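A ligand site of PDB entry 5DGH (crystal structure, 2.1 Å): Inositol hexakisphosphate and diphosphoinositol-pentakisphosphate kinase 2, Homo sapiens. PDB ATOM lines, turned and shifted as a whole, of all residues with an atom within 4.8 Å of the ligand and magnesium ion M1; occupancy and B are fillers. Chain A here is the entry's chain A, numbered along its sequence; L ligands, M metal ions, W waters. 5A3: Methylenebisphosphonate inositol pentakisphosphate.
An oxygen (O22) of the ligand is in salt-bridge range of the side-chain amino group of Lys 18.
The side-chain hydroxyl of Tyr 214 is in hydrogen-bond range of an oxygen (O31) of the ligand (2.6 Å).
The side-chain amino group of Lys 178 is in salt-bridge range of an oxygen (O26) of the ligand.
An oxygen (O31) of the ligand is in salt-bridge range of the side-chain amino group (NZ) of Lys 293.
NE of Arg 177 lies within salt-bridge range of O23 of the ligand, at 2.9 Å.
The side-chain amino group (NZ) of Lys 17 lies within salt-bridge range of an oxygen (O24) of the ligand (3.0 Å).
The guanidinium group (NH1) of Arg 226 lies within salt-bridge range of an oxygen (O41) of the ligand, at 3.0 Å.
O42 of the ligand lies within hydrogen-bond range of OG of Ser 290, at 3.0 Å.
An oxygen (O65) of the ligand lies within salt-bridge range of the guanidinium group of Arg 237 (3.1 Å).
OE1 of Glu 243 is in salt-bridge range of NZ of Lys 178, at 3.6 Å.
The side-chain amino group of Lys 293 is in hydrogen-bond range of the side-chain hydroxyl of Ser 290 (3.2 Å).
O of Phe 291 lies within hydrogen-bond range of NZ of Lys 293, at 2.8 Å.
The guanidinium group of Arg 177 is in hydrogen-bond range of a ring nitrogen (NE2) of His 158.
The guanidinium group (NH1) of Arg 226 lies within salt-bridge range of the side-chain carboxylate (OE1) of Glu 243, 3.4 Å away.
NH1 of Arg 237 sits at hydrogen-bond distance from O of Gly 241 (3.1 Å).
Lys 212 touches the ligand.
Hydrophobic or aromatic side chains that line the ligand: Tyr 214.
Of the 17 residues printed, 10 come within 4 Å of the ligand.
No residue comes within 4 Å of magnesium ion M1.
Water W5 is bound to magnesium ion M1 (2.0 Å).
Magnesium ion M1 is bound by water W2, at 2.1 Å.
O35 of the ligand binds magnesium ion M1 (2.1 Å).
Magnesium ion M1 is bound by an oxygen (O44) of the ligand.
Water W4 binds magnesium ion M1, 2.3 Å away.
Magnesium ion M1 has five donor atoms within binding distance.
Slightly farther from magnesium ion M1 lies water W10 (2.8 Å).
Water W2 lies within hydrogen-bond range of O of Lys 178 (2.7 Å) and O25 of the ligand (2.8 Å).
Water W3 lies within hydrogen-bond range of NZ of Lys 18 (2.6 Å), O34 of the ligand (2.6 Å) and NZ of Lys 17 (3.1 Å).
Water W7 bridges an oxygen (O43) of the ligand and the side-chain amino group of Lys 17.
Water W9 lies within hydrogen-bond range of O22 of the ligand (2.8 Å) and O of Phe 289 (2.9 Å).
Water W12 lies within hydrogen-bond range of a ring nitrogen (NE2) of His 158 (2.7 Å) and an oxygen (O33) of the ligand (2.8 Å).
Water W14 bridges NH2 of Arg 177 (3.2 Å) and O33 of the ligand (3.5 Å).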
ATOM      1  N   LYS A  17      -7.977 -14.235  -3.322  1.00  0.00           N
ATOM      2  CA  LYS A  17      -9.082 -14.707  -2.500  1.00  0.00           C
ATOM      3  C   LYS A  17     -10.276 -15.099  -3.402  1.00  0.00           C
ATOM      4  O   LYS A  17     -11.054 -15.991  -3.070  1.00  0.00           O
ATOM      5  CB  LYS A  17      -9.467 -13.623  -1.485  1.00  0.00           C
ATOM      6  CG  LYS A  17     -10.500 -14.051  -0.452  1.00  0.00           C
ATOM      7  CD  LYS A  17     -10.332 -13.260   0.846  1.00  0.00           C
ATOM      8  CE  LYS A  17     -11.665 -13.089   1.584  1.00  0.00           C
ATOM      9  NZ  LYS A  17     -12.405 -11.894   1.093  1.00  0.00           N
ATOM     10  N   LYS A  18     -10.380 -14.432  -4.554  1.00  0.00           N
ATOM     11  CA  LYS A  18     -11.388 -14.737  -5.553  1.00  0.00           C
ATOM     12  C   LYS A  18     -10.913 -15.808  -6.560  1.00  0.00           C
ATOM     13  O   LYS A  18     -11.656 -16.724  -6.892  1.00  0.00           O
ATOM     14  CB  LYS A  18     -11.815 -13.455  -6.258  1.00  0.00           C
ATOM     15  CG  LYS A  18     -12.146 -12.278  -5.326  1.00  0.00           C
ATOM     16  CD  LYS A  18     -13.292 -12.612  -4.383  1.00  0.00           C
ATOM     17  CE  LYS A  18     -13.869 -11.375  -3.682  1.00  0.00           C
ATOM     18  NZ  LYS A  18     -14.872 -11.730  -2.643  1.00  0.00           N
ATOM     19  N   SER A  66     -12.494  -6.406  -6.559  1.00  0.00           N
ATOM     20  CA  SER A  66     -12.961  -6.631  -5.191  1.00  0.00           C
ATOM     21  C   SER A  66     -11.984  -5.889  -4.318  1.00  0.00           C
ATOM     22  O   SER A  66     -11.011  -5.317  -4.841  1.00  0.00           O
ATOM     23  CB  SER A  66     -12.993  -8.122  -4.839  1.00  0.00           C
ATOM     24  OG  SER A  66     -11.724  -8.710  -4.999  1.00  0.00           O
ATOM     25  N   HIS A 158     -20.731  -2.300   3.758  1.00  0.00           N
ATOM     26  CA  HIS A 158     -21.902  -3.132   4.093  1.00  0.00           C
ATOM     27  C   HIS A 158     -22.599  -2.734   5.418  1.00  0.00           C
ATOM     28  O   HIS A 158     -23.471  -3.443   5.917  1.00  0.00           O
ATOM     29  CB  HIS A 158     -21.519  -4.632   4.012  1.00  0.00           C
ATOM     30  CG  HIS A 158     -20.924  -5.003   2.675  1.00  0.00           C
ATOM     31  ND1 HIS A 158     -21.660  -4.952   1.517  1.00  0.00           N
ATOM     32  CD2 HIS A 158     -19.656  -5.332   2.320  1.00  0.00           C
ATOM     33  CE1 HIS A 158     -20.883  -5.283   0.495  1.00  0.00           C
ATOM     34  NE2 HIS A 158     -19.664  -5.508   0.946  1.00  0.00           N
ATOM     35  N   ARG A 177     -21.063  -7.188   6.918  1.00  0.00           N
ATOM     36  CA  ARG A 177     -20.541  -8.358   6.256  1.00  0.00           C
ATOM     37  C   ARG A 177     -20.426  -9.395   7.368  1.00  0.00           C
ATOM     38  O   ARG A 177     -19.784  -9.146   8.389  1.00  0.00           O
ATOM     39  CB  ARG A 177     -19.202  -8.012   5.552  1.00  0.00           C
ATOM     40  CG  ARG A 177     -18.389  -9.155   4.928  1.00  0.00           C
ATOM     41  CD  ARG A 177     -19.091  -9.968   3.833  1.00  0.00           C
ATOM     42  NE  ARG A 177     -19.178  -9.295   2.521  1.00  0.00           N
ATOM     43  CZ  ARG A 177     -20.324  -8.872   1.977  1.00  0.00           C
ATOM     44  NH1 ARG A 177     -21.470  -9.036   2.649  1.00  0.00           N
ATOM     45  NH2 ARG A 177     -20.344  -8.302   0.787  1.00  0.00           N
ATOM     46  N   LYS A 178     -21.154 -10.502   7.168  1.00  0.00           N
ATOM     47  CA  LYS A 178     -21.205 -11.705   8.015  1.00  0.00           C
ATOM     48  C   LYS A 178     -19.972 -11.960   8.896  1.00  0.00           C
ATOM     49  O   LYS A 178     -18.866 -12.059   8.388  1.00  0.00           O
ATOM     50  CB  LYS A 178     -21.381 -12.923   7.102  1.00  0.00           C
ATOM     51  CG  LYS A 178     -22.463 -13.901   7.490  1.00  0.00           C
ATOM     52  CD  LYS A 178     -23.090 -14.539   6.249  1.00  0.00           C
ATOM     53  CE  LYS A 178     -22.122 -15.463   5.531  1.00  0.00           C
ATOM     54  NZ  LYS A 178     -22.111 -15.214   4.059  1.00  0.00           N
ATOM     55  N   LYS A 212     -31.306 -13.857  -4.195  1.00  0.00           N
ATOM     56  CA  LYS A 212     -30.006 -13.592  -4.768  1.00  0.00           C
ATOM     57  C   LYS A 212     -29.933 -14.192  -6.174  1.00  0.00           C
ATOM     58  O   LYS A 212     -30.129 -15.403  -6.355  1.00  0.00           O
ATOM     59  CB  LYS A 212     -28.951 -14.172  -3.855  1.00  0.00           C
ATOM     60  CG  LYS A 212     -28.969 -13.513  -2.472  1.00  0.00           C
ATOM     61  CD  LYS A 212     -27.918 -14.085  -1.557  1.00  0.00           C
ATOM     62  CE  LYS A 212     -26.630 -13.271  -1.593  1.00  0.00           C
ATOM     63  NZ  LYS A 212     -26.945 -11.815  -1.388  1.00  0.00           N
ATOM     64  N   TYR A 214     -27.877 -14.748  -9.890  1.00  0.00           N
ATOM     65  CA  TYR A 214     -26.550 -14.877 -10.448  1.00  0.00           C
ATOM     66  C   TYR A 214     -26.711 -15.147 -11.951  1.00  0.00           C
ATOM     67  O   TYR A 214     -27.230 -16.197 -12.329  1.00  0.00           O
ATOM     68  CB  TYR A 214     -25.815 -16.037  -9.788  1.00  0.00           C
ATOM     69  CG  TYR A 214     -25.621 -15.922  -8.290  1.00  0.00           C
ATOM     70  CD1 TYR A 214     -26.668 -16.211  -7.413  1.00  0.00           C
ATOM     71  CD2 TYR A 214     -24.395 -15.568  -7.751  1.00  0.00           C
ATOM     72  CE1 TYR A 214     -26.499 -16.143  -6.035  1.00  0.00           C
ATOM     73  CE2 TYR A 214     -24.206 -15.477  -6.378  1.00  0.00           C
ATOM     74  CZ  TYR A 214     -25.260 -15.764  -5.530  1.00  0.00           C
ATOM     75  OH  TYR A 214     -25.098 -15.688  -4.160  1.00  0.00           O
ATOM     76  N   ARG A 226     -32.190 -16.404   0.852  1.00  0.00           N
ATOM     77  CA  ARG A 226     -31.625 -16.552   2.197  1.00  0.00           C
ATOM     78  C   ARG A 226     -32.372 -15.624   3.104  1.00  0.00           C
ATOM     79  O   ARG A 226     -32.947 -14.648   2.652  1.00  0.00           O
ATOM     80  CB  ARG A 226     -30.148 -16.181   2.234  1.00  0.00           C
ATOM     81  CG  ARG A 226     -29.279 -17.146   1.448  1.00  0.00           C
ATOM     82  CD  ARG A 226     -27.835 -16.715   1.497  1.00  0.00           C
ATOM     83  NE  ARG A 226     -27.048 -17.443   0.516  1.00  0.00           N
ATOM     84  CZ  ARG A 226     -25.840 -17.062   0.097  1.00  0.00           C
ATOM     85  NH1 ARG A 226     -25.289 -15.960   0.593  1.00  0.00           N
ATOM     86  NH2 ARG A 226     -25.197 -17.780  -0.814  1.00  0.00           N
ATOM     87  N   ARG A 237     -27.030 -21.746   9.611  1.00  0.00           N
ATOM     88  CA  ARG A 237     -25.971 -22.545   8.989  1.00  0.00           C
ATOM     89  C   ARG A 237     -26.304 -24.044   9.006  1.00  0.00           C
ATOM     90  O   ARG A 237     -27.023 -24.514   9.901  1.00  0.00           O
ATOM     91  CB  ARG A 237     -24.602 -22.242   9.601  1.00  0.00           C
ATOM     92  CG  ARG A 237     -24.068 -20.855   9.245  1.00  0.00           C
ATOM     93  CD  ARG A 237     -22.599 -20.657   9.607  1.00  0.00           C
ATOM     94  NE  ARG A 237     -22.199 -19.243   9.506  1.00  0.00           N
ATOM     95  CZ  ARG A 237     -21.615 -18.676   8.444  1.00  0.00           C
ATOM     96  NH1 ARG A 237     -21.341 -19.403   7.362  1.00  0.00           N
ATOM     97  NH2 ARG A 237     -21.284 -17.395   8.469  1.00  0.00           N
ATOM     98  N   GLY A 241     -21.536 -25.902   8.181  1.00  0.00           N
ATOM     99  CA  GLY A 241     -21.200 -24.513   8.500  1.00  0.00           C
ATOM    100  C   GLY A 241     -21.406 -23.534   7.358  1.00  0.00           C
ATOM    101  O   GLY A 241     -20.867 -22.425   7.371  1.00  0.00           O
ATOM    102  N   GLU A 243     -24.120 -21.216   5.024  1.00  0.00           N
ATOM    103  CA  GLU A 243     -25.401 -20.536   5.212  1.00  0.00           C
ATOM    104  C   GLU A 243     -26.517 -21.267   4.481  1.00  0.00           C
ATOM    105  O   GLU A 243     -26.350 -21.645   3.330  1.00  0.00           O
ATOM    106  CB  GLU A 243     -25.314 -19.085   4.740  1.00  0.00           C
ATOM    107  CG  GLU A 243     -26.601 -18.301   4.915  1.00  0.00           C
ATOM    108  CD  GLU A 243     -26.407 -16.813   4.737  1.00  0.00           C
ATOM    109  OE1 GLU A 243     -25.550 -16.422   3.925  1.00  0.00           O
ATOM    110  OE2 GLU A 243     -27.116 -16.033   5.379  1.00  0.00           O
ATOM    111  N   ASN A 287     -24.173  -6.366  -7.485  1.00  0.00           N
ATOM    112  CA  ASN A 287     -22.829  -6.601  -6.985  1.00  0.00           C
ATOM    113  C   ASN A 287     -21.775  -6.780  -8.063  1.00  0.00           C
ATOM    114  O   ASN A 287     -20.601  -6.623  -7.789  1.00  0.00           O
ATOM    115  CB  ASN A 287     -22.819  -7.766  -5.987  1.00  0.00           C
ATOM    116  CG  ASN A 287     -23.565  -7.430  -4.724  1.00  0.00           C
ATOM    117  OD1 ASN A 287     -23.374  -6.341  -4.174  1.00  0.00           O
ATOM    118  ND2 ASN A 287     -24.441  -8.321  -4.253  1.00  0.00           N
ATOM    119  N   PHE A 289     -19.490  -9.138 -10.518  1.00  0.00           N
ATOM    120  CA  PHE A 289     -19.024 -10.530 -10.678  1.00  0.00           C
ATOM    121  C   PHE A 289     -19.220 -11.350  -9.421  1.00  0.00           C
ATOM    122  O   PHE A 289     -18.697 -11.003  -8.352  1.00  0.00           O
ATOM    123  CB  PHE A 289     -17.543 -10.544 -11.095  1.00  0.00           C
ATOM    124  CG  PHE A 289     -17.073 -11.873 -11.626  1.00  0.00           C
ATOM    125  CD1 PHE A 289     -16.811 -12.932 -10.752  1.00  0.00           C
ATOM    126  CD2 PHE A 289     -16.900 -12.067 -12.987  1.00  0.00           C
ATOM    127  CE1 PHE A 289     -16.375 -14.163 -11.228  1.00  0.00           C
ATOM    128  CE2 PHE A 289     -16.456 -13.293 -13.465  1.00  0.00           C
ATOM    129  CZ  PHE A 289     -16.193 -14.338 -12.601  1.00  0.00           C
ATOM    130  N   SER A 290     -19.956 -12.453  -9.546  1.00  0.00           N
ATOM    131  CA  SER A 290     -20.176 -13.357  -8.453  1.00  0.00           C
ATOM    132  C   SER A 290     -20.624 -14.714  -8.958  1.00  0.00           C
ATOM    133  O   SER A 290     -21.451 -14.800  -9.849  1.00  0.00           O
ATOM    134  CB  SER A 290     -21.201 -12.785  -7.467  1.00  0.00           C
ATOM    135  OG  SER A 290     -21.290 -13.606  -6.312  1.00  0.00           O
ATOM    136  N   PHE A 291     -20.054 -15.765  -8.373  1.00  0.00           N
ATOM    137  CA  PHE A 291     -20.442 -17.154  -8.657  1.00  0.00           C
ATOM    138  C   PHE A 291     -21.408 -17.701  -7.595  1.00  0.00           C
ATOM    139  O   PHE A 291     -21.314 -17.348  -6.412  1.00  0.00           O
ATOM    140  CB  PHE A 291     -19.197 -18.070  -8.691  1.00  0.00           C
ATOM    141  CG  PHE A 291     -18.334 -17.909  -9.909  1.00  0.00           C
ATOM    142  CD1 PHE A 291     -18.882 -17.632 -11.159  1.00  0.00           C
ATOM    143  CD2 PHE A 291     -16.952 -18.067  -9.810  1.00  0.00           C
ATOM    144  CE1 PHE A 291     -18.083 -17.503 -12.278  1.00  0.00           C
ATOM    145  CE2 PHE A 291     -16.146 -17.955 -10.942  1.00  0.00           C
ATOM    146  CZ  PHE A 291     -16.706 -17.689 -12.168  1.00  0.00           C
ATOM    147  N   LYS A 293     -22.253 -20.440  -5.013  1.00  0.00           N
ATOM    148  CA  LYS A 293     -21.383 -21.302  -4.189  1.00  0.00           C
ATOM    149  C   LYS A 293     -22.043 -22.658  -3.932  1.00  0.00           C
ATOM    150  O   LYS A 293     -23.235 -22.747  -3.659  1.00  0.00           O
ATOM    151  CB  LYS A 293     -21.065 -20.632  -2.864  1.00  0.00           C
ATOM    152  CG  LYS A 293     -20.145 -19.413  -2.927  1.00  0.00           C
ATOM    153  CD  LYS A 293     -20.869 -18.118  -3.293  1.00  0.00           C
ATOM    154  CE  LYS A 293     -19.888 -16.953  -3.386  1.00  0.00           C
ATOM    155  NZ  LYS A 293     -20.459 -15.825  -4.184  1.00  0.00           N
HETATM  156  O31 5A3 L   1     -22.829 -14.668  -3.361  1.00  0.00           O
HETATM  157  C2  5A3 L   1     -19.082 -12.395  -1.394  1.00  0.00           C
HETATM  158  C1  5A3 L   1     -20.236 -13.284  -0.838  1.00  0.00           C
HETATM  159  C4  5A3 L   1     -17.746 -12.868   0.713  1.00  0.00           C
HETATM  160  C5  5A3 L   1     -18.856 -13.770   1.226  1.00  0.00           C
HETATM  161  C6  5A3 L   1     -19.753 -14.347   0.153  1.00  0.00           C
HETATM  162  C3  5A3 L   1     -18.260 -11.781  -0.248  1.00  0.00           C
HETATM  163  O11 5A3 L   1     -20.862 -13.999  -1.917  1.00  0.00           O
HETATM  164  O75 5A3 L   1     -16.935 -17.567   5.494  1.00  0.00           O
HETATM  165  PB5 5A3 L   1     -18.555 -17.495   5.278  1.00  0.00           P
HETATM  166  O55 5A3 L   1     -19.111 -19.009   5.271  1.00  0.00           O
HETATM  167  O65 5A3 L   1     -19.240 -16.647   6.290  1.00  0.00           O
HETATM  168  CB5 5A3 L   1     -18.891 -16.904   3.562  1.00  0.00           C
HETATM  169  PA5 5A3 L   1     -18.361 -15.088   3.372  1.00  0.00           P
HETATM  170  O25 5A3 L   1     -19.412 -14.047   4.087  1.00  0.00           O
HETATM  171  O35 5A3 L   1     -16.952 -14.975   4.120  1.00  0.00           O
HETATM  172  O15 5A3 L   1     -18.205 -14.843   1.798  1.00  0.00           O
HETATM  173  O16 5A3 L   1     -20.904 -14.972   0.794  1.00  0.00           O
HETATM  174  PA6 5A3 L   1     -21.232 -16.564   0.650  1.00  0.00           P
HETATM  175  O46 5A3 L   1     -22.241 -16.585  -0.439  1.00  0.00           O
HETATM  176  O36 5A3 L   1     -19.965 -17.257   0.371  1.00  0.00           O
HETATM  177  O26 5A3 L   1     -21.774 -16.873   1.993  1.00  0.00           O
HETATM  178  PA1 5A3 L   1     -22.455 -13.789  -2.227  1.00  0.00           P
HETATM  179  O41 5A3 L   1     -23.215 -14.385  -0.923  1.00  0.00           O
HETATM  180  O21 5A3 L   1     -22.637 -12.310  -2.356  1.00  0.00           O
HETATM  181  O12 5A3 L   1     -18.217 -13.163  -2.253  1.00  0.00           O
HETATM  182  PA2 5A3 L   1     -18.195 -12.927  -3.864  1.00  0.00           P
HETATM  183  O42 5A3 L   1     -19.495 -12.336  -4.224  1.00  0.00           O
HETATM  184  O22 5A3 L   1     -17.021 -12.064  -4.054  1.00  0.00           O
HETATM  185  O32 5A3 L   1     -18.014 -14.317  -4.310  1.00  0.00           O
HETATM  186  O13 5A3 L   1     -17.117 -11.072  -0.810  1.00  0.00           O
HETATM  187  PA3 5A3 L   1     -16.846  -9.507  -0.569  1.00  0.00           P
HETATM  188  O43 5A3 L   1     -15.542  -9.274  -1.207  1.00  0.00           O
HETATM  189  O33 5A3 L   1     -18.002  -8.886  -1.204  1.00  0.00           O
HETATM  190  O23 5A3 L   1     -16.809  -9.409   0.929  1.00  0.00           O
HETATM  191  O14 5A3 L   1     -17.192 -12.242   1.869  1.00  0.00           O
HETATM  192  PA4 5A3 L   1     -15.641 -12.240   2.284  1.00  0.00           P
HETATM  193  O24 5A3 L   1     -15.160 -10.944   1.823  1.00  0.00           O
HETATM  194  O44 5A3 L   1     -15.750 -12.404   3.756  1.00  0.00           O
HETATM  195  O34 5A3 L   1     -15.000 -13.406   1.580  1.00  0.00           O
HETATM  196 MG    MG M   1     -16.177 -13.677   5.550  1.00  0.00          MG
HETATM  197 MG    MG M   2     -17.937  -7.662  -5.432  1.00  0.00          MG
HETATM  198  O   HOH W   1     -17.724 -15.265  -6.879  1.00  0.00           O
HETATM  199  O   HOH W   2     -17.867 -12.541   5.922  1.00  0.00           O
HETATM  200  O   HOH W   3     -14.079 -13.502  -0.889  1.00  0.00           O
HETATM  201  O   HOH W   4     -15.089 -12.312   7.107  1.00  0.00           O
HETATM  202  O   HOH W   5     -16.551 -15.015   6.995  1.00  0.00           O
HETATM  203  O   HOH W   6     -14.751  -6.811  -2.119  1.00  0.00           O
HETATM  204  O   HOH W   7     -12.823  -9.427  -0.781  1.00  0.00           O
HETATM  205  O   HOH W   8     -15.485 -16.106   2.026  1.00  0.00           O
HETATM  206  O   HOH W   9     -16.428 -11.263  -6.640  1.00  0.00           O
HETATM  207  O   HOH W  10     -14.254 -15.305   4.264  1.00  0.00           O
HETATM  208  O   HOH W  11     -17.982  -9.306  -3.623  1.00  0.00           O
HETATM  209  O   HOH W  12     -17.772  -6.132  -0.937  1.00  0.00           O
HETATM  210  O   HOH W  13     -21.044 -10.135  -3.973  1.00  0.00           O
HETATM  211  O   HOH W  14     -21.121  -7.757  -2.295  1.00  0.00           O
